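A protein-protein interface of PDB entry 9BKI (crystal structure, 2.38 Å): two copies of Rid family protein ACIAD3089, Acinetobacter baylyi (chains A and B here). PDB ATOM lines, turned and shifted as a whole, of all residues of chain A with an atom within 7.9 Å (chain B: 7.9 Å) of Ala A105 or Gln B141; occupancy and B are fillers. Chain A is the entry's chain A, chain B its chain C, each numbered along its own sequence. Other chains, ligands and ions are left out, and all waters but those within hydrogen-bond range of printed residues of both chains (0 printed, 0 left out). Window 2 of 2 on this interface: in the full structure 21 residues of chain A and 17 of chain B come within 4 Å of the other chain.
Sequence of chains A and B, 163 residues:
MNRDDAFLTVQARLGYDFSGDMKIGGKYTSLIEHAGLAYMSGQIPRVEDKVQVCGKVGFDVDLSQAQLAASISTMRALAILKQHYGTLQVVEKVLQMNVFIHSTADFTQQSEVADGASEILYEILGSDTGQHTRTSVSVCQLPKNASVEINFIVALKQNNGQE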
ATOM      1  N   LYS A  56     -20.031  31.413   4.354  1.00  0.00           N
ATOM      2  CA  LYS A  56     -19.178  30.553   3.555  1.00  0.00           C
ATOM      3  C   LYS A  56     -19.919  29.251   3.261  1.00  0.00           C
ATOM      4  O   LYS A  56     -20.259  28.504   4.185  1.00  0.00           O
ATOM      5  CB  LYS A  56     -17.860  30.330   4.300  1.00  0.00           C
ATOM      6  CG  LYS A  56     -16.774  29.622   3.531  1.00  0.00           C
ATOM      7  CD  LYS A  56     -15.398  29.787   4.200  1.00  0.00           C
ATOM      8  CE  LYS A  56     -15.374  29.463   5.697  1.00  0.00           C
ATOM      9  NZ  LYS A  56     -13.965  29.562   6.266  1.00  0.00           N
ATOM     10  N   VAL A  57     -20.205  29.001   1.981  1.00  0.00           N
ATOM     11  CA  VAL A  57     -20.890  27.769   1.600  1.00  0.00           C
ATOM     12  C   VAL A  57     -20.045  26.581   2.015  1.00  0.00           C
ATOM     13  O   VAL A  57     -18.836  26.544   1.769  1.00  0.00           O
ATOM     14  CB  VAL A  57     -21.172  27.753   0.093  1.00  0.00           C
ATOM     15  CG1 VAL A  57     -21.848  26.444  -0.313  1.00  0.00           C
ATOM     16  CG2 VAL A  57     -22.022  28.941  -0.286  1.00  0.00           C
ATOM     17  N   GLY A  58     -20.672  25.614   2.674  1.00  0.00           N
ATOM     18  CA  GLY A  58     -19.948  24.511   3.259  1.00  0.00           C
ATOM     19  C   GLY A  58     -19.501  24.740   4.688  1.00  0.00           C
ATOM     20  O   GLY A  58     -18.939  23.823   5.303  1.00  0.00           O
ATOM     21  N   ILE A 101     -18.577  31.222  -6.073  1.00  0.00           N
ATOM     22  CA  ILE A 101     -19.186  30.733  -4.842  1.00  0.00           C
ATOM     23  C   ILE A 101     -18.178  30.863  -3.711  1.00  0.00           C
ATOM     24  O   ILE A 101     -17.129  30.214  -3.725  1.00  0.00           O
ATOM     25  CB  ILE A 101     -19.678  29.282  -4.969  1.00  0.00           C
ATOM     26  CG1 ILE A 101     -20.710  29.167  -6.097  1.00  0.00           C
ATOM     27  CG2 ILE A 101     -20.301  28.837  -3.628  1.00  0.00           C
ATOM     28  CD1 ILE A 101     -20.856  27.792  -6.682  1.00  0.00           C
ATOM     29  N   SER A 103     -16.867  29.648  -0.692  1.00  0.00           N
ATOM     30  CA  SER A 103     -17.010  28.326  -0.092  1.00  0.00           C
ATOM     31  C   SER A 103     -15.724  27.906   0.613  1.00  0.00           C
ATOM     32  O   SER A 103     -14.675  28.554   0.501  1.00  0.00           O
ATOM     33  CB  SER A 103     -17.371  27.269  -1.139  1.00  0.00           C
ATOM     34  OG  SER A 103     -16.200  26.809  -1.800  1.00  0.00           O
ATOM     35  N   THR A 104     -15.825  26.795   1.350  1.00  0.00           N
ATOM     36  CA  THR A 104     -14.680  26.136   1.967  1.00  0.00           C
ATOM     37  C   THR A 104     -13.873  25.379   0.911  1.00  0.00           C
ATOM     38  O   THR A 104     -14.262  25.285  -0.261  1.00  0.00           O
ATOM     39  CB  THR A 104     -15.122  25.156   3.043  1.00  0.00           C
ATOM     40  OG1 THR A 104     -15.870  24.092   2.440  1.00  0.00           O
ATOM     41  CG2 THR A 104     -15.987  25.839   4.082  1.00  0.00           C
ATOM     42  N   ALA A 105     -12.735  24.826   1.341  1.00  0.00           N
ATOM     43  CA  ALA A 105     -11.871  24.033   0.464  1.00  0.00           C
ATOM     44  C   ALA A 105     -12.332  22.596   0.301  1.00  0.00           C
ATOM     45  O   ALA A 105     -11.715  21.857  -0.467  1.00  0.00           O
ATOM     46  CB  ALA A 105     -10.429  24.045   0.976  1.00  0.00           C
ATOM     47  N   ASP A 106     -13.427  22.200   0.937  1.00  0.00           N
ATOM     48  CA  ASP A 106     -13.978  20.861   0.806  1.00  0.00           C
ATOM     49  C   ASP A 106     -15.243  20.818  -0.031  1.00  0.00           C
ATOM     50  O   ASP A 106     -15.721  19.728  -0.345  1.00  0.00           O
ATOM     51  CB  ASP A 106     -14.311  20.305   2.194  1.00  0.00           C
ATOM     52  CG  ASP A 106     -13.098  20.205   3.067  1.00  0.00           C
ATOM     53  OD1 ASP A 106     -12.092  19.657   2.588  1.00  0.00           O
ATOM     54  OD2 ASP A 106     -13.134  20.716   4.210  1.00  0.00           O
ATOM     55  N   PHE A 107     -15.828  21.969  -0.335  1.00  0.00           N
ATOM     56  CA  PHE A 107     -17.086  22.021  -1.060  1.00  0.00           C
ATOM     57  C   PHE A 107     -16.849  21.693  -2.534  1.00  0.00           C
ATOM     58  O   PHE A 107     -15.962  22.268  -3.171  1.00  0.00           O
ATOM     59  CB  PHE A 107     -17.698  23.413  -0.888  1.00  0.00           C
ATOM     60  CG  PHE A 107     -19.050  23.565  -1.500  1.00  0.00           C
ATOM     61  CD1 PHE A 107     -20.158  22.994  -0.915  1.00  0.00           C
ATOM     62  CD2 PHE A 107     -19.207  24.288  -2.668  1.00  0.00           C
ATOM     63  CE1 PHE A 107     -21.410  23.133  -1.489  1.00  0.00           C
ATOM     64  CE2 PHE A 107     -20.448  24.428  -3.253  1.00  0.00           C
ATOM     65  CZ  PHE A 107     -21.558  23.850  -2.661  1.00  0.00           C
ATOM     66  N   THR A 108     -17.611  20.727  -3.061  1.00  0.00           N
ATOM     67  CA  THR A 108     -17.446  20.275  -4.436  1.00  0.00           C
ATOM     68  C   THR A 108     -18.748  20.325  -5.226  1.00  0.00           C
ATOM     69  O   THR A 108     -18.805  19.782  -6.333  1.00  0.00           O
ATOM     70  CB  THR A 108     -16.869  18.854  -4.500  1.00  0.00           C
ATOM     71  OG1 THR A 108     -17.738  17.953  -3.800  1.00  0.00           O
ATOM     72  CG2 THR A 108     -15.481  18.820  -3.862  1.00  0.00           C
ATOM     73  N   GLN A 109     -19.789  20.965  -4.700  1.00  0.00           N
ATOM     74  CA  GLN A 109     -21.084  20.974  -5.370  1.00  0.00           C
ATOM     75  C   GLN A 109     -21.359  22.296  -6.056  1.00  0.00           C
ATOM     76  O   GLN A 109     -22.490  22.791  -6.034  1.00  0.00           O
ATOM     77  CB  GLN A 109     -22.193  20.619  -4.380  1.00  0.00           C
ATOM     78  CG  GLN A 109     -22.232  19.121  -4.042  1.00  0.00           C
ATOM     79  CD  GLN A 109     -23.115  18.788  -2.855  1.00  0.00           C
ATOM     80  OE1 GLN A 109     -23.001  19.382  -1.782  1.00  0.00           O
ATOM     81  NE2 GLN A 109     -24.049  17.876  -3.067  1.00  0.00           N
ATOM     82  N   GLN A 110     -20.346  22.864  -6.722  1.00  0.00           N
ATOM     83  CA  GLN A 110     -20.536  24.138  -7.410  1.00  0.00           C
ATOM     84  C   GLN A 110     -21.630  24.046  -8.471  1.00  0.00           C
ATOM     85  O   GLN A 110     -22.411  24.988  -8.639  1.00  0.00           O
ATOM     86  CB  GLN A 110     -19.219  24.618  -8.030  1.00  0.00           C
ATOM     87  CG  GLN A 110     -18.138  25.056  -7.027  1.00  0.00           C
ATOM     88  CD  GLN A 110     -17.394  23.884  -6.393  1.00  0.00           C
ATOM     89  OE1 GLN A 110     -17.682  22.723  -6.664  1.00  0.00           O
ATOM     90  NE2 GLN A 110     -16.424  24.193  -5.550  1.00  0.00           N
ATOM     91  N   SER A 136     -18.628  27.901 -13.103  1.00  0.00           N
ATOM     92  CA  SER A 136     -18.965  27.865 -11.680  1.00  0.00           C
ATOM     93  C   SER A 136     -17.724  27.470 -10.892  1.00  0.00           C
ATOM     94  O   SER A 136     -17.276  26.329 -10.991  1.00  0.00           O
ATOM     95  CB  SER A 136     -20.096  26.873 -11.439  1.00  0.00           C
ATOM     96  OG  SER A 136     -20.579  26.970 -10.126  1.00  0.00           O
ATOM     97  N   VAL A 137     -17.175  28.386 -10.096  1.00  0.00           N
ATOM     98  CA  VAL A 137     -15.944  28.123  -9.361  1.00  0.00           C
ATOM     99  C   VAL A 137     -16.121  28.612  -7.936  1.00  0.00           C
ATOM    100  O   VAL A 137     -16.970  29.456  -7.647  1.00  0.00           O
ATOM    101  CB  VAL A 137     -14.723  28.804 -10.015  1.00  0.00           C
ATOM    102  CG1 VAL A 137     -14.631  28.432 -11.497  1.00  0.00           C
ATOM    103  CG2 VAL A 137     -14.818  30.315  -9.863  1.00  0.00           C
ATOM    104  N   SER A 138     -15.305  28.067  -7.031  1.00  0.00           N
ATOM    105  CA  SER A 138     -15.314  28.506  -5.639  1.00  0.00           C
ATOM    106  C   SER A 138     -14.245  29.564  -5.446  1.00  0.00           C
ATOM    107  O   SER A 138     -13.117  29.409  -5.924  1.00  0.00           O
ATOM    108  CB  SER A 138     -15.070  27.358  -4.665  1.00  0.00           C
ATOM    109  OG  SER A 138     -16.233  26.591  -4.473  1.00  0.00           O
ATOM    110  N   VAL A 139     -14.608  30.644  -4.766  1.00  0.00           N
ATOM    111  CA  VAL A 139     -13.686  31.715  -4.458  1.00  0.00           C
ATOM    112  C   VAL A 139     -13.549  31.832  -2.953  1.00  0.00           C
ATOM    113  O   VAL A 139     -14.360  31.326  -2.177  1.00  0.00           O
ATOM    114  CB  VAL A 139     -14.116  33.056  -5.078  1.00  0.00           C
ATOM    115  CG1 VAL A 139     -14.029  32.965  -6.605  1.00  0.00           C
ATOM    116  CG2 VAL A 139     -15.527  33.451  -4.595  1.00  0.00           C
ATOM    117  N   CYS A 140     -12.532  32.588  -2.561  1.00  0.00           N
ATOM    118  CA  CYS A 140     -12.103  32.694  -1.177  1.00  0.00           C
ATOM    119  C   CYS A 140     -12.928  33.699  -0.369  1.00  0.00           C
ATOM    120  O   CYS A 140     -13.044  33.560   0.853  1.00  0.00           O
ATOM    121  CB  CYS A 140     -10.613  33.054  -1.222  1.00  0.00           C
ATOM    122  SG  CYS A 140      -9.966  33.899   0.151  1.00  0.00           S
ATOM    123  N   GLY B  55      -7.700  17.148  -7.348  1.00  0.00           N
ATOM    124  CA  GLY B  55      -6.914  17.562  -6.210  1.00  0.00           C
ATOM    125  C   GLY B  55      -6.510  19.012  -6.298  1.00  0.00           C
ATOM    126  O   GLY B  55      -6.871  19.743  -7.220  1.00  0.00           O
ATOM    127  N   LYS B  56      -5.737  19.420  -5.314  1.00  0.00           N
ATOM    128  CA  LYS B  56      -5.309  20.795  -5.125  1.00  0.00           C
ATOM    129  C   LYS B  56      -3.877  20.924  -5.609  1.00  0.00           C
ATOM    130  O   LYS B  56      -2.985  20.249  -5.087  1.00  0.00           O
ATOM    131  CB  LYS B  56      -5.447  21.187  -3.649  1.00  0.00           C
ATOM    132  CG  LYS B  56      -5.143  22.630  -3.316  1.00  0.00           C
ATOM    133  CD  LYS B  56      -5.688  23.032  -1.918  1.00  0.00           C
ATOM    134  CE  LYS B  56      -5.347  22.064  -0.787  1.00  0.00           C
ATOM    135  NZ  LYS B  56      -5.889  22.549   0.532  1.00  0.00           N
ATOM    136  N   PHE B 100      -8.894  28.744 -14.357  1.00  0.00           N
ATOM    137  CA  PHE B 100      -9.092  28.772 -12.915  1.00  0.00           C
ATOM    138  C   PHE B 100      -8.429  27.531 -12.337  1.00  0.00           C
ATOM    139  O   PHE B 100      -8.784  26.406 -12.700  1.00  0.00           O
ATOM    140  CB  PHE B 100     -10.585  28.798 -12.565  1.00  0.00           C
ATOM    141  CG  PHE B 100     -11.333  29.962 -13.152  1.00  0.00           C
ATOM    142  CD1 PHE B 100     -11.359  31.187 -12.501  1.00  0.00           C
ATOM    143  CD2 PHE B 100     -12.028  29.829 -14.352  1.00  0.00           C
ATOM    144  CE1 PHE B 100     -12.070  32.273 -13.043  1.00  0.00           C
ATOM    145  CE2 PHE B 100     -12.732  30.892 -14.888  1.00  0.00           C
ATOM    146  CZ  PHE B 100     -12.755  32.122 -14.235  1.00  0.00           C
ATOM    147  N   ILE B 101      -7.508  27.727 -11.414  1.00  0.00           N
ATOM    148  CA  ILE B 101      -6.652  26.653 -10.930  1.00  0.00           C
ATOM    149  C   ILE B 101      -6.935  26.430  -9.449  1.00  0.00           C
ATOM    150  O   ILE B 101      -6.718  27.324  -8.622  1.00  0.00           O
ATOM    151  CB  ILE B 101      -5.176  26.999 -11.165  1.00  0.00           C
ATOM    152  CG1 ILE B 101      -4.944  27.270 -12.670  1.00  0.00           C
ATOM    153  CG2 ILE B 101      -4.296  25.901 -10.670  1.00  0.00           C
ATOM    154  CD1 ILE B 101      -3.757  28.123 -12.946  1.00  0.00           C
ATOM    155  N   HIS B 102      -7.392  25.236  -9.113  1.00  0.00           N
ATOM    156  CA  HIS B 102      -7.622  24.833  -7.727  1.00  0.00           C
ATOM    157  C   HIS B 102      -6.278  24.537  -7.080  1.00  0.00           C
ATOM    158  O   HIS B 102      -5.697  23.472  -7.298  1.00  0.00           O
ATOM    159  CB  HIS B 102      -8.517  23.605  -7.712  1.00  0.00           C
ATOM    160  CG  HIS B 102      -8.718  23.011  -6.358  1.00  0.00           C
ATOM    161  ND1 HIS B 102      -9.303  21.775  -6.182  1.00  0.00           N
ATOM    162  CD2 HIS B 102      -8.432  23.476  -5.119  1.00  0.00           C
ATOM    163  CE1 HIS B 102      -9.353  21.498  -4.894  1.00  0.00           C
ATOM    164  NE2 HIS B 102      -8.836  22.515  -4.228  1.00  0.00           N
ATOM    165  N   SER B 103      -5.789  25.449  -6.243  1.00  0.00           N
ATOM    166  CA  SER B 103      -4.430  25.362  -5.723  1.00  0.00           C
ATOM    167  C   SER B 103      -4.369  25.814  -4.269  1.00  0.00           C
ATOM    168  O   SER B 103      -5.339  26.324  -3.710  1.00  0.00           O
ATOM    169  CB  SER B 103      -3.467  26.208  -6.562  1.00  0.00           C
ATOM    170  OG  SER B 103      -3.529  27.558  -6.161  1.00  0.00           O
ATOM    171  N   SER B 138      -5.729  31.479  -9.228  1.00  0.00           N
ATOM    172  CA  SER B 138      -5.952  30.353  -8.338  1.00  0.00           C
ATOM    173  C   SER B 138      -7.275  30.527  -7.609  1.00  0.00           C
ATOM    174  O   SER B 138      -7.581  31.614  -7.110  1.00  0.00           O
ATOM    175  CB  SER B 138      -4.810  30.201  -7.334  1.00  0.00           C
ATOM    176  OG  SER B 138      -3.685  29.571  -7.931  1.00  0.00           O
ATOM    177  N   VAL B 139      -8.061  29.456  -7.567  1.00  0.00           N
ATOM    178  CA  VAL B 139      -9.332  29.444  -6.872  1.00  0.00           C
ATOM    179  C   VAL B 139      -9.287  28.424  -5.741  1.00  0.00           C
ATOM    180  O   VAL B 139      -8.406  27.560  -5.652  1.00  0.00           O
ATOM    181  CB  VAL B 139     -10.508  29.159  -7.822  1.00  0.00           C
ATOM    182  CG1 VAL B 139     -10.648  30.310  -8.796  1.00  0.00           C
ATOM    183  CG2 VAL B 139     -10.266  27.858  -8.581  1.00  0.00           C
ATOM    184  N   CYS B 140     -10.294  28.518  -4.896  1.00  0.00           N
ATOM    185  CA  CYS B 140     -10.332  27.772  -3.656  1.00  0.00           C
ATOM    186  C   CYS B 140     -10.860  26.348  -3.844  1.00  0.00           C
ATOM    187  O   CYS B 140     -10.448  25.440  -3.116  1.00  0.00           O
ATOM    188  CB  CYS B 140     -11.179  28.618  -2.693  1.00  0.00           C
ATOM    189  SG  CYS B 140     -11.991  27.827  -1.411  1.00  0.00           S
ATOM    190  N   GLN B 141     -11.705  26.114  -4.843  1.00  0.00           N
ATOM    191  CA  GLN B 141     -12.233  24.779  -5.114  1.00  0.00           C
ATOM    192  C   GLN B 141     -12.913  24.807  -6.469  1.00  0.00           C
ATOM    193  O   GLN B 141     -13.147  25.875  -7.043  1.00  0.00           O
ATOM    194  CB  GLN B 141     -13.206  24.288  -4.033  1.00  0.00           C
ATOM    195  CG  GLN B 141     -12.601  23.198  -3.131  1.00  0.00           C
ATOM    196  CD  GLN B 141     -12.420  21.858  -3.861  1.00  0.00           C
ATOM    197  OE1 GLN B 141     -12.648  21.760  -5.068  1.00  0.00           O
ATOM    198  NE2 GLN B 141     -12.020  20.821  -3.125  1.00  0.00           N
ATOM    199  N   LEU B 142     -13.202  23.620  -6.984  1.00  0.00           N
ATOM    200  CA  LEU B 142     -13.769  23.464  -8.312  1.00  0.00           C
ATOM    201  C   LEU B 142     -14.786  22.339  -8.292  1.00  0.00           C
ATOM    202  O   LEU B 142     -14.756  21.487  -7.397  1.00  0.00           O
ATOM    203  CB  LEU B 142     -12.682  23.180  -9.360  1.00  0.00           C
ATOM    204  CG  LEU B 142     -11.830  24.380  -9.757  1.00  0.00           C
ATOM    205  CD1 LEU B 142     -10.743  23.953 -10.746  1.00  0.00           C
ATOM    206  CD2 LEU B 142     -12.753  25.473 -10.357  1.00  0.00           C
ATOM    207  N   PRO B 143     -15.705  22.309  -9.261  1.00  0.00           N
ATOM    208  CA  PRO B 143     -16.680  21.211  -9.312  1.00  0.00           C
ATOM    209  C   PRO B 143     -15.982  19.856  -9.248  1.00  0.00           C
ATOM    210  O   PRO B 143     -14.966  19.627  -9.919  1.00  0.00           O
ATOM    211  CB  PRO B 143     -17.375  21.414 -10.666  1.00  0.00           C
ATOM    212  CG  PRO B 143     -17.188  22.878 -10.999  1.00  0.00           C
ATOM    213  CD  PRO B 143     -15.876  23.271 -10.378  1.00  0.00           C
ATOM    214  N   LYS B 144     -16.534  18.959  -8.426  1.00  0.00           N
ATOM    215  CA  LYS B 144     -16.090  17.570  -8.316  1.00  0.00           C
ATOM    216  C   LYS B 144     -14.614  17.488  -7.913  1.00  0.00           C
ATOM    217  O   LYS B 144     -13.916  16.523  -8.236  1.00  0.00           O
ATOM    218  CB  LYS B 144     -16.348  16.819  -9.634  1.00  0.00           C
ATOM    219  CG  LYS B 144     -17.857  16.659 -10.029  1.00  0.00           C
ATOM    220  CD  LYS B 144     -18.689  16.089  -8.884  1.00  0.00           C
ATOM    221  CE  LYS B 144     -20.127  16.645  -8.868  1.00  0.00           C
ATOM    222  NZ  LYS B 144     -20.697  16.793  -7.473  1.00  0.00           N
ATOM    223  N   ASN B 145     -14.129  18.484  -7.171  1.00  0.00           N
ATOM    224  CA  ASN B 145     -12.746  18.505  -6.693  1.00  0.00           C
ATOM    225  C   ASN B 145     -11.724  18.536  -7.845  1.00  0.00           C
ATOM    226  O   ASN B 145     -10.582  18.096  -7.680  1.00  0.00           O
ATOM    227  CB  ASN B 145     -12.489  17.300  -5.781  1.00  0.00           C
ATOM    228  CG  ASN B 145     -11.234  17.441  -4.933  1.00  0.00           C
ATOM    229  OD1 ASN B 145     -10.947  18.495  -4.358  1.00  0.00           O
ATOM    230  ND2 ASN B 145     -10.482  16.372  -4.852  1.00  0.00           N
ATOM    231  N   ALA B 146     -12.110  19.057  -9.017  1.00  0.00           N
ATOM    232  CA  ALA B 146     -11.191  19.159 -10.151  1.00  0.00           C
ATOM    233  C   ALA B 146     -10.032  20.089  -9.834  1.00  0.00           C
ATOM    234  O   ALA B 146     -10.109  20.949  -8.951  1.00  0.00           O
ATOM    235  CB  ALA B 146     -11.892  19.681 -11.403  1.00  0.00           C
ATOM    236  N   SER B 147      -8.947  19.919 -10.581  1.00  0.00           N
ATOM    237  CA  SER B 147      -7.766  20.746 -10.362  1.00  0.00           C
ATOM    238  C   SER B 147      -7.716  21.978 -11.247  1.00  0.00           C
ATOM    239  O   SER B 147      -7.053  22.949 -10.872  1.00  0.00           O
ATOM    240  CB  SER B 147      -6.487  19.947 -10.611  1.00  0.00           C
ATOM    241  OG  SER B 147      -6.452  19.544 -11.957  1.00  0.00           O
ATOM    242  N   GLU B 149     -10.156  24.418 -14.279  1.00  0.00           N
ATOM    243  CA  GLU B 149     -11.355  24.646 -15.081  1.00  0.00           C
ATOM    244  C   GLU B 149     -11.093  25.809 -16.038  1.00  0.00           C
ATOM    245  O   GLU B 149     -10.572  26.852 -15.631  1.00  0.00           O
ATOM    246  CB  GLU B 149     -12.590  24.948 -14.205  1.00  0.00           C
ATOM    247  CG  GLU B 149     -13.875  24.990 -15.047  1.00  0.00           C
ATOM    248  CD  GLU B 149     -15.130  25.330 -14.280  1.00  0.00           C
ATOM    249  OE1 GLU B 149     -15.212  25.113 -13.045  1.00  0.00           O
ATOM    250  OE2 GLU B 149     -16.053  25.847 -14.934  1.00  0.00           O
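The backbone carbonyl oxygen of Ser A136 sits close to the side-chain carboxylate of Glu B149, at 3.2 Å.
OE1 of Gln A110 sits close to N of Pro B143 (3.3 Å).
N of Ser A138 lies within hydrogen-bond range of O of Gln B141 (3.1 Å).
O of Leu B142 sits close to OE1 of Gln A110.
The backbone carbonyl oxygen (O) of Ala A105 is in hydrogen-bond range of the side-chain amide nitrogen (NE2) of Gln B141.
The backbone carbonyl oxygen of Thr A104 lies within hydrogen-bond range of the side-chain sulfur of Cys B140 (3.6 Å).
SG of Cys B140 is in hydrogen-bond range of O of Ser A103.
The backbone carbonyl oxygen (O) of Thr A108 lies within hydrogen-bond range of the backbone NH (N) of Lys B144 (3.2 Å).
The backbone NH of Cys B140 lies within hydrogen-bond range of the backbone carbonyl oxygen of Ser A138 (3.1 Å).
The backbone carbonyl oxygen (O) of Asn B145 lies within hydrogen-bond range of the backbone NH (N) of Gly B55, 3.1 Å away.
The backbone carbonyl oxygen of Glu B149 is in hydrogen-bond range of the backbone NH of Phe B100, 2.8 Å away.
The backbone NH of Ile A101 lies within hydrogen-bond range of the backbone carbonyl oxygen of Val A137 (2.9 Å).
O of Val A57 sits at hydrogen-bond distance from N of Thr A104.
The side-chain amide oxygen (OD1) of Asn B145 lies within hydrogen-bond range of the side-chain amide nitrogen (NE2) of Gln B141, 2.8 Å away.
The backbone carbonyl oxygen (O) of Ile B101 is in hydrogen-bond range of the backbone NH (N) of Val B139, at 2.7 Å.
Among the printed residues, pairs that only touch across the chains: Ser A138 with Val B139 (3.2 Å), Ser A136 with Pro B143 (3.4 Å), Phe A107 with Gln B141 (3.5 Å), Gln A110 with Gln B141 (3.6 Å), Thr A108 with Asn B145 (3.6 Å), Val A137 with Leu B142 (3.7 Å), Val A137 with Glu B149 (3.7 Å), Thr A104 with Gln B141 (3.9 Å), Thr A108 with Pro B143 (3.9 Å) and Val A137 with Phe B100 (3.99 Å).
Of chain B, only Gln B141 (2.9 Å) comes within 4 Å of Ala A105.
Printed residues of chain B within 4 Å of Gln A110: Gln B141, Leu B142 and Pro B143.
Gly B55 touches none of the printed residues of chain A.
Ile B101 touches none of the printed residues of chain A.
Of the printed residues of chain A, Cys B140 touches Ser A103 (3.4 Å), Thr A104 (3.6 Å) and Ser A138 (3.1 Å).
Gln B141 touches just these residues of chain A: Thr A104, Ala A105, Phe A107, Gln A110 and Ser A138.
Of the printed residues of chain A, Pro B143 touches Thr A108 (3.9 Å), Gln A110 (3.2 Å) and Ser A136 (3.4 Å).
Printed residues of chain A within 4 Å of Asn B145: Thr A108.
The nearest residue of chain A that does not touch Gln B141 is Thr A108 (4.1 Å).
The nearest printed residue of chain B that does not touch Gln A110 is Lys B144 (4.3 Å).
Of the 17 printed residues of chain A, 9 touch a printed residue of chain B.
Hydrophobic or aromatic side chains of chain A within 4 Å of the printed part of chain B: Val A137.
Among the printed residues, 19 pairs touch across the chains.
Among the printed residues, no Asp or Glu carboxylate lies within 4 Å of a Lys or Arg side-chain nitrogen of the other chain.
Ser A103 touches Cys B140, but with the chains exchanged Cys A140 does not touch Ser B103 (8.9 Å).
Ser A138 touches Val B139, but with the chains exchanged Val A139 does not touch Ser B138 (6.6 Å).
Ser A138 touches Cys B140, but with the chains exchanged Cys A140 does not touch Ser B138 (6.8 Å).
Positions printed for both chains: 56, 101, 103, 138, 139 and 140.
Of the 19 pairs that touch across the chains among the printed residues, none has its exchanged pair printed and touching as well.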
